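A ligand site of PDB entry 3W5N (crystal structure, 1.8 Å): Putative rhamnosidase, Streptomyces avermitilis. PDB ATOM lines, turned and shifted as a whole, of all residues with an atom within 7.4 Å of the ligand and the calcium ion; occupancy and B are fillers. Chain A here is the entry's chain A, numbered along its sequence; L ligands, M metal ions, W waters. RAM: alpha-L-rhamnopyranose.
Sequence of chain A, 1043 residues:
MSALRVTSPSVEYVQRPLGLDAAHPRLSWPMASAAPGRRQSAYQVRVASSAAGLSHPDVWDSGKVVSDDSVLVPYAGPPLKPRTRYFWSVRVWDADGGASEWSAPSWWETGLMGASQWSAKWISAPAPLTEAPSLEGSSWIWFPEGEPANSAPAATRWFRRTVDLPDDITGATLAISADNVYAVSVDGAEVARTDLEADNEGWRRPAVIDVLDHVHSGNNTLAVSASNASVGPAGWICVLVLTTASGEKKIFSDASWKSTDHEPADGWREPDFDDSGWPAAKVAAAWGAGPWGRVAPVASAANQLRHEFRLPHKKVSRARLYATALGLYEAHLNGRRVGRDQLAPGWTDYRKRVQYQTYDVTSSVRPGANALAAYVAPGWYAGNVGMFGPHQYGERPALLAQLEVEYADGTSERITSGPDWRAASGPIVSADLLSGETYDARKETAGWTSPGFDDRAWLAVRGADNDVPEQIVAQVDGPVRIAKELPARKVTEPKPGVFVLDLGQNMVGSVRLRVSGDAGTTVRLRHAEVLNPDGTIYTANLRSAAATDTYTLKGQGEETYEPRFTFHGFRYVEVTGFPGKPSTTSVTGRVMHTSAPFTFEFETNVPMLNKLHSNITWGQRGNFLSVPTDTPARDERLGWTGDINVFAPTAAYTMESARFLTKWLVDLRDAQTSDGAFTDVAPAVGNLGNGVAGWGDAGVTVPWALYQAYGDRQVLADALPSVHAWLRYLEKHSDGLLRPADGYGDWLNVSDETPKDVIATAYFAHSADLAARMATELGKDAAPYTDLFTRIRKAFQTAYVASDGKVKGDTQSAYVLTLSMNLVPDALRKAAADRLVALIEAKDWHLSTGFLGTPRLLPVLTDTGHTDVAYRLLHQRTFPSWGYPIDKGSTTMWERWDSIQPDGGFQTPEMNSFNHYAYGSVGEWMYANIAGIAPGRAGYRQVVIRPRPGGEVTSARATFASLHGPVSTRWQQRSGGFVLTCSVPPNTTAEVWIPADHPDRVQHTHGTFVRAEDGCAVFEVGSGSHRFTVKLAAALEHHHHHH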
ATOM      1  N   PRO A 148      12.444  27.081  19.420  1.00  0.00           N
ATOM      2  CA  PRO A 148      13.696  27.416  20.121  1.00  0.00           C
ATOM      3  C   PRO A 148      13.740  27.007  21.588  1.00  0.00           C
ATOM      4  O   PRO A 148      14.831  26.743  22.108  1.00  0.00           O
ATOM      5  CB  PRO A 148      13.808  28.946  19.956  1.00  0.00           C
ATOM      6  CG  PRO A 148      12.981  29.267  18.758  1.00  0.00           C
ATOM      7  CD  PRO A 148      11.823  28.278  18.805  1.00  0.00           C
ATOM      8  N   ALA A 149      12.592  26.916  22.257  1.00  0.00           N
ATOM      9  CA  ALA A 149      12.599  26.500  23.668  1.00  0.00           C
ATOM     10  C   ALA A 149      13.046  25.026  23.811  1.00  0.00           C
ATOM     11  O   ALA A 149      13.499  24.595  24.886  1.00  0.00           O
ATOM     12  CB  ALA A 149      11.221  26.714  24.301  1.00  0.00           C
ATOM     13  N   ASN A 150      12.936  24.279  22.721  1.00  0.00           N
ATOM     14  CA  ASN A 150      13.412  22.894  22.692  1.00  0.00           C
ATOM     15  C   ASN A 150      14.814  22.799  22.095  1.00  0.00           C
ATOM     16  O   ASN A 150      15.731  22.235  22.712  1.00  0.00           O
ATOM     17  CB  ASN A 150      12.428  21.983  21.937  1.00  0.00           C
ATOM     18  CG  ASN A 150      12.884  20.536  21.905  1.00  0.00           C
ATOM     19  OD1 ASN A 150      13.427  20.061  20.906  1.00  0.00           O
ATOM     20  ND2 ASN A 150      12.715  19.832  23.038  1.00  0.00           N
ATOM     21  N   ALA A 152      17.636  24.998  19.214  1.00  0.00           N
ATOM     22  CA  ALA A 152      18.014  25.997  18.234  1.00  0.00           C
ATOM     23  C   ALA A 152      19.477  25.737  17.930  1.00  0.00           C
ATOM     24  O   ALA A 152      20.176  25.109  18.746  1.00  0.00           O
ATOM     25  CB  ALA A 152      17.811  27.401  18.810  1.00  0.00           C
ATOM     26  N   PRO A 153      19.954  26.183  16.750  1.00  0.00           N
ATOM     27  CA  PRO A 153      21.379  25.982  16.414  1.00  0.00           C
ATOM     28  C   PRO A 153      22.297  26.811  17.324  1.00  0.00           C
ATOM     29  O   PRO A 153      21.844  27.786  17.944  1.00  0.00           O
ATOM     30  CB  PRO A 153      21.472  26.489  14.964  1.00  0.00           C
ATOM     31  CG  PRO A 153      20.309  27.400  14.794  1.00  0.00           C
ATOM     32  CD  PRO A 153      19.224  26.815  15.634  1.00  0.00           C
ATOM     33  N   ALA A 178      19.587  36.001  28.931  1.00  0.00           N
ATOM     34  CA  ALA A 178      19.619  35.247  27.676  1.00  0.00           C
ATOM     35  C   ALA A 178      20.135  33.849  27.906  1.00  0.00           C
ATOM     36  O   ALA A 178      21.062  33.631  28.701  1.00  0.00           O
ATOM     37  CB  ALA A 178      20.491  35.952  26.634  1.00  0.00           C
ATOM     38  N   ASP A 179      19.527  32.905  27.197  1.00  0.00           N
ATOM     39  CA  ASP A 179      20.068  31.588  26.973  1.00  0.00           C
ATOM     40  C   ASP A 179      20.678  31.633  25.555  1.00  0.00           C
ATOM     41  O   ASP A 179      19.942  31.517  24.580  1.00  0.00           O
ATOM     42  CB  ASP A 179      18.928  30.565  27.052  1.00  0.00           C
ATOM     43  CG  ASP A 179      19.386  29.150  26.815  1.00  0.00           C
ATOM     44  OD1 ASP A 179      20.534  28.964  26.384  1.00  0.00           O
ATOM     45  OD2 ASP A 179      18.609  28.203  27.073  1.00  0.00           O
ATOM     46  N   ASN A 180      22.004  31.812  25.405  1.00  0.00           N
ATOM     47  CA  ASN A 180      22.993  31.818  26.496  1.00  0.00           C
ATOM     48  C   ASN A 180      23.639  33.155  26.851  1.00  0.00           C
ATOM     49  O   ASN A 180      23.985  33.376  28.027  1.00  0.00           O
ATOM     50  CB  ASN A 180      24.111  30.798  26.186  1.00  0.00           C
ATOM     51  CG  ASN A 180      23.628  29.380  26.327  1.00  0.00           C
ATOM     52  OD1 ASN A 180      23.296  28.711  25.333  1.00  0.00           O
ATOM     53  ND2 ASN A 180      23.525  28.911  27.572  1.00  0.00           N
ATOM     54  N   VAL A 181      23.826  34.036  25.872  1.00  0.00           N
ATOM     55  CA  VAL A 181      24.485  35.331  26.129  1.00  0.00           C
ATOM     56  C   VAL A 181      23.866  36.439  25.270  1.00  0.00           C
ATOM     57  O   VAL A 181      23.194  36.143  24.265  1.00  0.00           O
ATOM     58  CB  VAL A 181      26.023  35.285  25.867  1.00  0.00           C
ATOM     59  CG1 VAL A 181      26.720  34.320  26.826  1.00  0.00           C
ATOM     60  CG2 VAL A 181      26.340  34.955  24.413  1.00  0.00           C
ATOM     61  N   ASP A 199      30.074  32.075  30.585  1.00  0.00           N
ATOM     62  CA  ASP A 199      28.710  31.605  30.817  1.00  0.00           C
ATOM     63  C   ASP A 199      28.641  30.285  31.573  1.00  0.00           C
ATOM     64  O   ASP A 199      29.137  29.250  31.105  1.00  0.00           O
ATOM     65  CB  ASP A 199      27.916  31.493  29.514  1.00  0.00           C
ATOM     66  CG  ASP A 199      26.488  31.020  29.742  1.00  0.00           C
ATOM     67  OD1 ASP A 199      25.834  31.534  30.678  1.00  0.00           O
ATOM     68  OD2 ASP A 199      26.012  30.137  28.994  1.00  0.00           O
ATOM     69  N   ASN A 200      28.011  30.317  32.743  1.00  0.00           N
ATOM     70  CA  ASN A 200      27.611  29.099  33.422  1.00  0.00           C
ATOM     71  C   ASN A 200      26.123  29.138  33.790  1.00  0.00           C
ATOM     72  O   ASN A 200      25.774  29.492  34.923  1.00  0.00           O
ATOM     73  CB  ASN A 200      28.493  28.812  34.642  1.00  0.00           C
ATOM     74  CG  ASN A 200      28.566  27.330  34.955  1.00  0.00           C
ATOM     75  OD1 ASN A 200      27.560  26.696  35.297  1.00  0.00           O
ATOM     76  ND2 ASN A 200      29.771  26.764  34.826  1.00  0.00           N
ATOM     77  N   GLU A 201      25.270  28.794  32.828  1.00  0.00           N
ATOM     78  CA  GLU A 201      23.809  28.906  32.965  1.00  0.00           C
ATOM     79  C   GLU A 201      23.420  30.305  33.428  1.00  0.00           C
ATOM     80  O   GLU A 201      22.584  30.487  34.303  1.00  0.00           O
ATOM     81  CB  GLU A 201      23.234  27.804  33.872  1.00  0.00           C
ATOM     82  CG  GLU A 201      23.665  26.410  33.414  1.00  0.00           C
ATOM     83  CD  GLU A 201      22.960  25.268  34.127  1.00  0.00           C
ATOM     84  OE1 GLU A 201      22.243  25.493  35.127  1.00  0.00           O
ATOM     85  OE2 GLU A 201      23.149  24.114  33.681  1.00  0.00           O
ATOM     86  N   GLY A 202      24.079  31.294  32.815  1.00  0.00           N
ATOM     87  CA  GLY A 202      23.806  32.706  33.054  1.00  0.00           C
ATOM     88  C   GLY A 202      22.362  33.128  32.847  1.00  0.00           C
ATOM     89  O   GLY A 202      21.921  34.137  33.412  1.00  0.00           O
ATOM     90  N   TRP A 203      21.615  32.373  32.054  1.00  0.00           N
ATOM     91  CA  TRP A 203      20.195  32.622  31.850  1.00  0.00           C
ATOM     92  C   TRP A 203      19.390  32.624  33.152  1.00  0.00           C
ATOM     93  O   TRP A 203      18.355  33.266  33.237  1.00  0.00           O
ATOM     94  CB  TRP A 203      19.588  31.651  30.831  1.00  0.00           C
ATOM     95  CG  TRP A 203      19.704  30.177  31.169  1.00  0.00           C
ATOM     96  CD1 TRP A 203      20.637  29.303  30.713  1.00  0.00           C
ATOM     97  CD2 TRP A 203      18.835  29.431  32.033  1.00  0.00           C
ATOM     98  NE1 TRP A 203      20.408  28.037  31.238  1.00  0.00           N
ATOM     99  CE2 TRP A 203      19.305  28.099  32.039  1.00  0.00           C
ATOM    100  CE3 TRP A 203      17.684  29.761  32.764  1.00  0.00           C
ATOM    101  CZ2 TRP A 203      18.675  27.086  32.793  1.00  0.00           C
ATOM    102  CZ3 TRP A 203      17.063  28.751  33.516  1.00  0.00           C
ATOM    103  CH2 TRP A 203      17.554  27.449  33.518  1.00  0.00           C
ATOM    104  N   ARG A 204      19.884  31.894  34.160  1.00  0.00           N
ATOM    105  CA  ARG A 204      19.226  31.825  35.474  1.00  0.00           C
ATOM    106  C   ARG A 204      19.328  33.101  36.263  1.00  0.00           C
ATOM    107  O   ARG A 204      18.605  33.279  37.248  1.00  0.00           O
ATOM    108  CB  ARG A 204      19.852  30.730  36.341  1.00  0.00           C
ATOM    109  CG  ARG A 204      19.741  29.332  35.776  1.00  0.00           C
ATOM    110  CD  ARG A 204      20.467  28.354  36.673  1.00  0.00           C
ATOM    111  NE  ARG A 204      20.338  26.996  36.177  1.00  0.00           N
ATOM    112  CZ  ARG A 204      19.259  26.237  36.336  1.00  0.00           C
ATOM    113  NH1 ARG A 204      18.210  26.701  37.004  1.00  0.00           N
ATOM    114  NH2 ARG A 204      19.242  25.010  35.837  1.00  0.00           N
ATOM    115  N   SER A 227      23.396  34.894  21.585  1.00  0.00           N
ATOM    116  CA  SER A 227      24.010  33.698  21.050  1.00  0.00           C
ATOM    117  C   SER A 227      23.666  32.479  21.895  1.00  0.00           C
ATOM    118  O   SER A 227      23.604  32.542  23.127  1.00  0.00           O
ATOM    119  CB  SER A 227      25.529  33.848  20.964  1.00  0.00           C
ATOM    120  OG  SER A 227      25.882  34.988  20.196  1.00  0.00           O
ATOM    121  N   ASN A 228      23.449  31.367  21.203  1.00  0.00           N
ATOM    122  CA  ASN A 228      23.213  30.071  21.833  1.00  0.00           C
ATOM    123  C   ASN A 228      24.541  29.291  21.843  1.00  0.00           C
ATOM    124  O   ASN A 228      25.199  29.182  20.818  1.00  0.00           O
ATOM    125  CB  ASN A 228      22.157  29.322  21.010  1.00  0.00           C
ATOM    126  CG  ASN A 228      21.648  28.051  21.684  1.00  0.00           C
ATOM    127  OD1 ASN A 228      21.807  27.833  22.870  1.00  0.00           O
ATOM    128  ND2 ASN A 228      20.988  27.211  20.890  1.00  0.00           N
ATOM    129  N   ALA A 229      24.909  28.745  22.997  1.00  0.00           N
ATOM    130  CA  ALA A 229      26.267  28.202  23.184  1.00  0.00           C
ATOM    131  C   ALA A 229      26.490  26.835  22.543  1.00  0.00           C
ATOM    132  O   ALA A 229      27.628  26.478  22.199  1.00  0.00           O
ATOM    133  CB  ALA A 229      26.593  28.130  24.662  1.00  0.00           C
ATOM    134  N   SER A 230      25.423  26.075  22.398  1.00  0.00           N
ATOM    135  CA  SER A 230      25.487  24.745  21.809  1.00  0.00           C
ATOM    136  C   SER A 230      24.099  24.409  21.294  1.00  0.00           C
ATOM    137  O   SER A 230      23.128  25.070  21.663  1.00  0.00           O
ATOM    138  CB  SER A 230      25.928  23.716  22.850  1.00  0.00           C
ATOM    139  OG  SER A 230      24.933  23.540  23.845  1.00  0.00           O
ATOM    140  N   VAL A 231      23.989  23.365  20.474  1.00  0.00           N
ATOM    141  CA  VAL A 231      22.672  22.899  20.034  1.00  0.00           C
ATOM    142  C   VAL A 231      21.794  22.511  21.218  1.00  0.00           C
ATOM    143  O   VAL A 231      22.164  21.680  22.056  1.00  0.00           O
ATOM    144  CB  VAL A 231      22.787  21.739  19.031  1.00  0.00           C
ATOM    145  CG1 VAL A 231      21.415  21.294  18.564  1.00  0.00           C
ATOM    146  CG2 VAL A 231      23.630  22.156  17.837  1.00  0.00           C
ATOM    147  N   GLY A 232      20.616  23.128  21.289  1.00  0.00           N
ATOM    148  CA  GLY A 232      19.720  23.053  22.426  1.00  0.00           C
ATOM    149  C   GLY A 232      18.945  24.360  22.573  1.00  0.00           C
ATOM    150  O   GLY A 232      18.971  25.202  21.654  1.00  0.00           O
ATOM    151  N   PRO A 233      18.240  24.542  23.697  1.00  0.00           N
ATOM    152  CA  PRO A 233      17.313  25.680  23.836  1.00  0.00           C
ATOM    153  C   PRO A 233      17.994  27.038  23.711  1.00  0.00           C
ATOM    154  O   PRO A 233      19.156  27.181  24.085  1.00  0.00           O
ATOM    155  CB  PRO A 233      16.710  25.498  25.235  1.00  0.00           C
ATOM    156  CG  PRO A 233      16.974  24.073  25.605  1.00  0.00           C
ATOM    157  CD  PRO A 233      18.239  23.681  24.898  1.00  0.00           C
ATOM    158  N   ALA A 234      17.274  28.017  23.177  1.00  0.00           N
ATOM    159  CA  ALA A 234      17.772  29.379  23.070  1.00  0.00           C
ATOM    160  C   ALA A 234      16.613  30.343  23.238  1.00  0.00           C
ATOM    161  O   ALA A 234      15.450  30.019  22.901  1.00  0.00           O
ATOM    162  CB  ALA A 234      18.448  29.615  21.728  1.00  0.00           C
ATOM    163  N   GLY A 235      16.931  31.536  23.710  1.00  0.00           N
ATOM    164  CA  GLY A 235      15.914  32.555  23.879  1.00  0.00           C
ATOM    165  C   GLY A 235      16.450  33.663  24.761  1.00  0.00           C
ATOM    166  O   GLY A 235      17.349  33.435  25.560  1.00  0.00           O
ATOM    167  N   PRO A 291      12.086  25.606  29.173  1.00  0.00           N
ATOM    168  CA  PRO A 291      12.930  24.948  30.179  1.00  0.00           C
ATOM    169  C   PRO A 291      13.368  25.850  31.342  1.00  0.00           C
ATOM    170  O   PRO A 291      13.962  25.350  32.309  1.00  0.00           O
ATOM    171  CB  PRO A 291      14.144  24.510  29.371  1.00  0.00           C
ATOM    172  CG  PRO A 291      14.223  25.469  28.224  1.00  0.00           C
ATOM    173  CD  PRO A 291      12.799  25.828  27.899  1.00  0.00           C
ATOM    174  N   TRP A 292      13.072  27.149  31.251  1.00  0.00           N
ATOM    175  CA  TRP A 292      13.755  28.140  32.089  1.00  0.00           C
ATOM    176  C   TRP A 292      13.090  28.415  33.452  1.00  0.00           C
ATOM    177  O   TRP A 292      13.746  28.915  34.369  1.00  0.00           O
ATOM    178  CB  TRP A 292      13.960  29.436  31.311  1.00  0.00           C
ATOM    179  CG  TRP A 292      14.651  29.216  29.980  1.00  0.00           C
ATOM    180  CD1 TRP A 292      15.965  28.871  29.769  1.00  0.00           C
ATOM    181  CD2 TRP A 292      14.066  29.347  28.674  1.00  0.00           C
ATOM    182  NE1 TRP A 292      16.223  28.759  28.412  1.00  0.00           N
ATOM    183  CE2 TRP A 292      15.080  29.069  27.720  1.00  0.00           C
ATOM    184  CE3 TRP A 292      12.774  29.675  28.208  1.00  0.00           C
ATOM    185  CZ2 TRP A 292      14.852  29.088  26.338  1.00  0.00           C
ATOM    186  CZ3 TRP A 292      12.543  29.703  26.826  1.00  0.00           C
ATOM    187  CH2 TRP A 292      13.577  29.414  25.911  1.00  0.00           C
HETATM  188  C1  RAM L   1      21.776  24.559  30.184  1.00  0.00           C
HETATM  189  C2  RAM L   1      22.596  25.431  29.232  1.00  0.00           C
HETATM  190  C3  RAM L   1      21.913  25.508  27.851  1.00  0.00           C
HETATM  191  C4  RAM L   1      20.469  25.991  27.971  1.00  0.00           C
HETATM  192  C5  RAM L   1      19.686  25.079  28.922  1.00  0.00           C
HETATM  193  C6  RAM L   1      18.284  25.599  29.216  1.00  0.00           C
HETATM  194  O1  RAM L   1      21.880  23.190  29.776  1.00  0.00           O
HETATM  195  O2  RAM L   1      22.700  26.720  29.828  1.00  0.00           O
HETATM  196  O3  RAM L   1      22.586  26.333  26.878  1.00  0.00           O
HETATM  197  O4  RAM L   1      19.975  26.036  26.613  1.00  0.00           O
HETATM  198  O5  RAM L   1      20.379  24.936  30.188  1.00  0.00           O
HETATM  199 CA    CA M   1      21.335  27.208  25.085  1.00  0.00          CA
HETATM  200  O   HOH W   1      25.184  27.530  30.371  1.00  0.00           O
HETATM  201  O   HOH W   2      21.895  25.033  24.162  1.00  0.00           O
HETATM  202  O   HOH W   3      24.847  25.067  26.254  1.00  0.00           O
HETATM  203  O   HOH W   4      24.459  22.337  27.901  1.00  0.00           O
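Within 4 Å of the calcium ion: Asp 179, Asn 180, Asn 228 and Pro 233.
The nearest printed residue that does not touch the calcium ion is Ala 229 (4.4 Å).
The calcium ion is bound by OD1 of Asp 179 (2.3 Å), OD1 of Asn 228 (2.3 Å), O3 of the ligand (2.4 Å), O4 of the ligand (2.4 Å), O of Pro 233 (2.4 Å), water W2 (2.4 Å) and OD1 of Asn 180 (2.5 Å).
The calcium ion has seven donor atoms within binding distance.
Merely in contact with the ligand: Glu 201 and Trp 292.
Within 4 Å of the ligand: Asp 179, Asn 180, Glu 201, Trp 203, Pro 233 and Trp 292.
The nearest printed residue that does not touch the ligand is Pro 291 (4.2 Å).
The indole nitrogen (NE1) of Trp 203 sits at hydrogen-bond distance from an oxygen (O2) of the ligand.
OD2 of Asp 179 lies within hydrogen-bond range of NE1 of Trp 292 (2.8 Å).
N of Asp 179 is in hydrogen-bond range of O of Gly 235 (2.8 Å).
O of Ser 230 lies within hydrogen-bond range of ND2 of Asn 228, 3.1 Å away.
ND2 of Asn 228 lies within hydrogen-bond range of O of Gly 232 (2.9 Å).
The side-chain amide nitrogen of Asn 228 lies within hydrogen-bond range of the backbone carbonyl oxygen of Ala 152 (3.1 Å).
The side-chain amide nitrogen (ND2) of Asn 228 sits at hydrogen-bond distance from the backbone carbonyl oxygen (O) of Pro 153 (3.1 Å).
OD1 of Asn 180 sits close to N of Ala 229 (2.8 Å).
The side-chain carboxylate (OE1) of Glu 201 is in salt-bridge range of the guanidinium group (NE) of Arg 204 (2.6 Å).
Water W1 lies within hydrogen-bond range of an oxygen (O2) of the ligand, the backbone NH of Glu 201 and the side-chain carboxylate of Asp 199.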
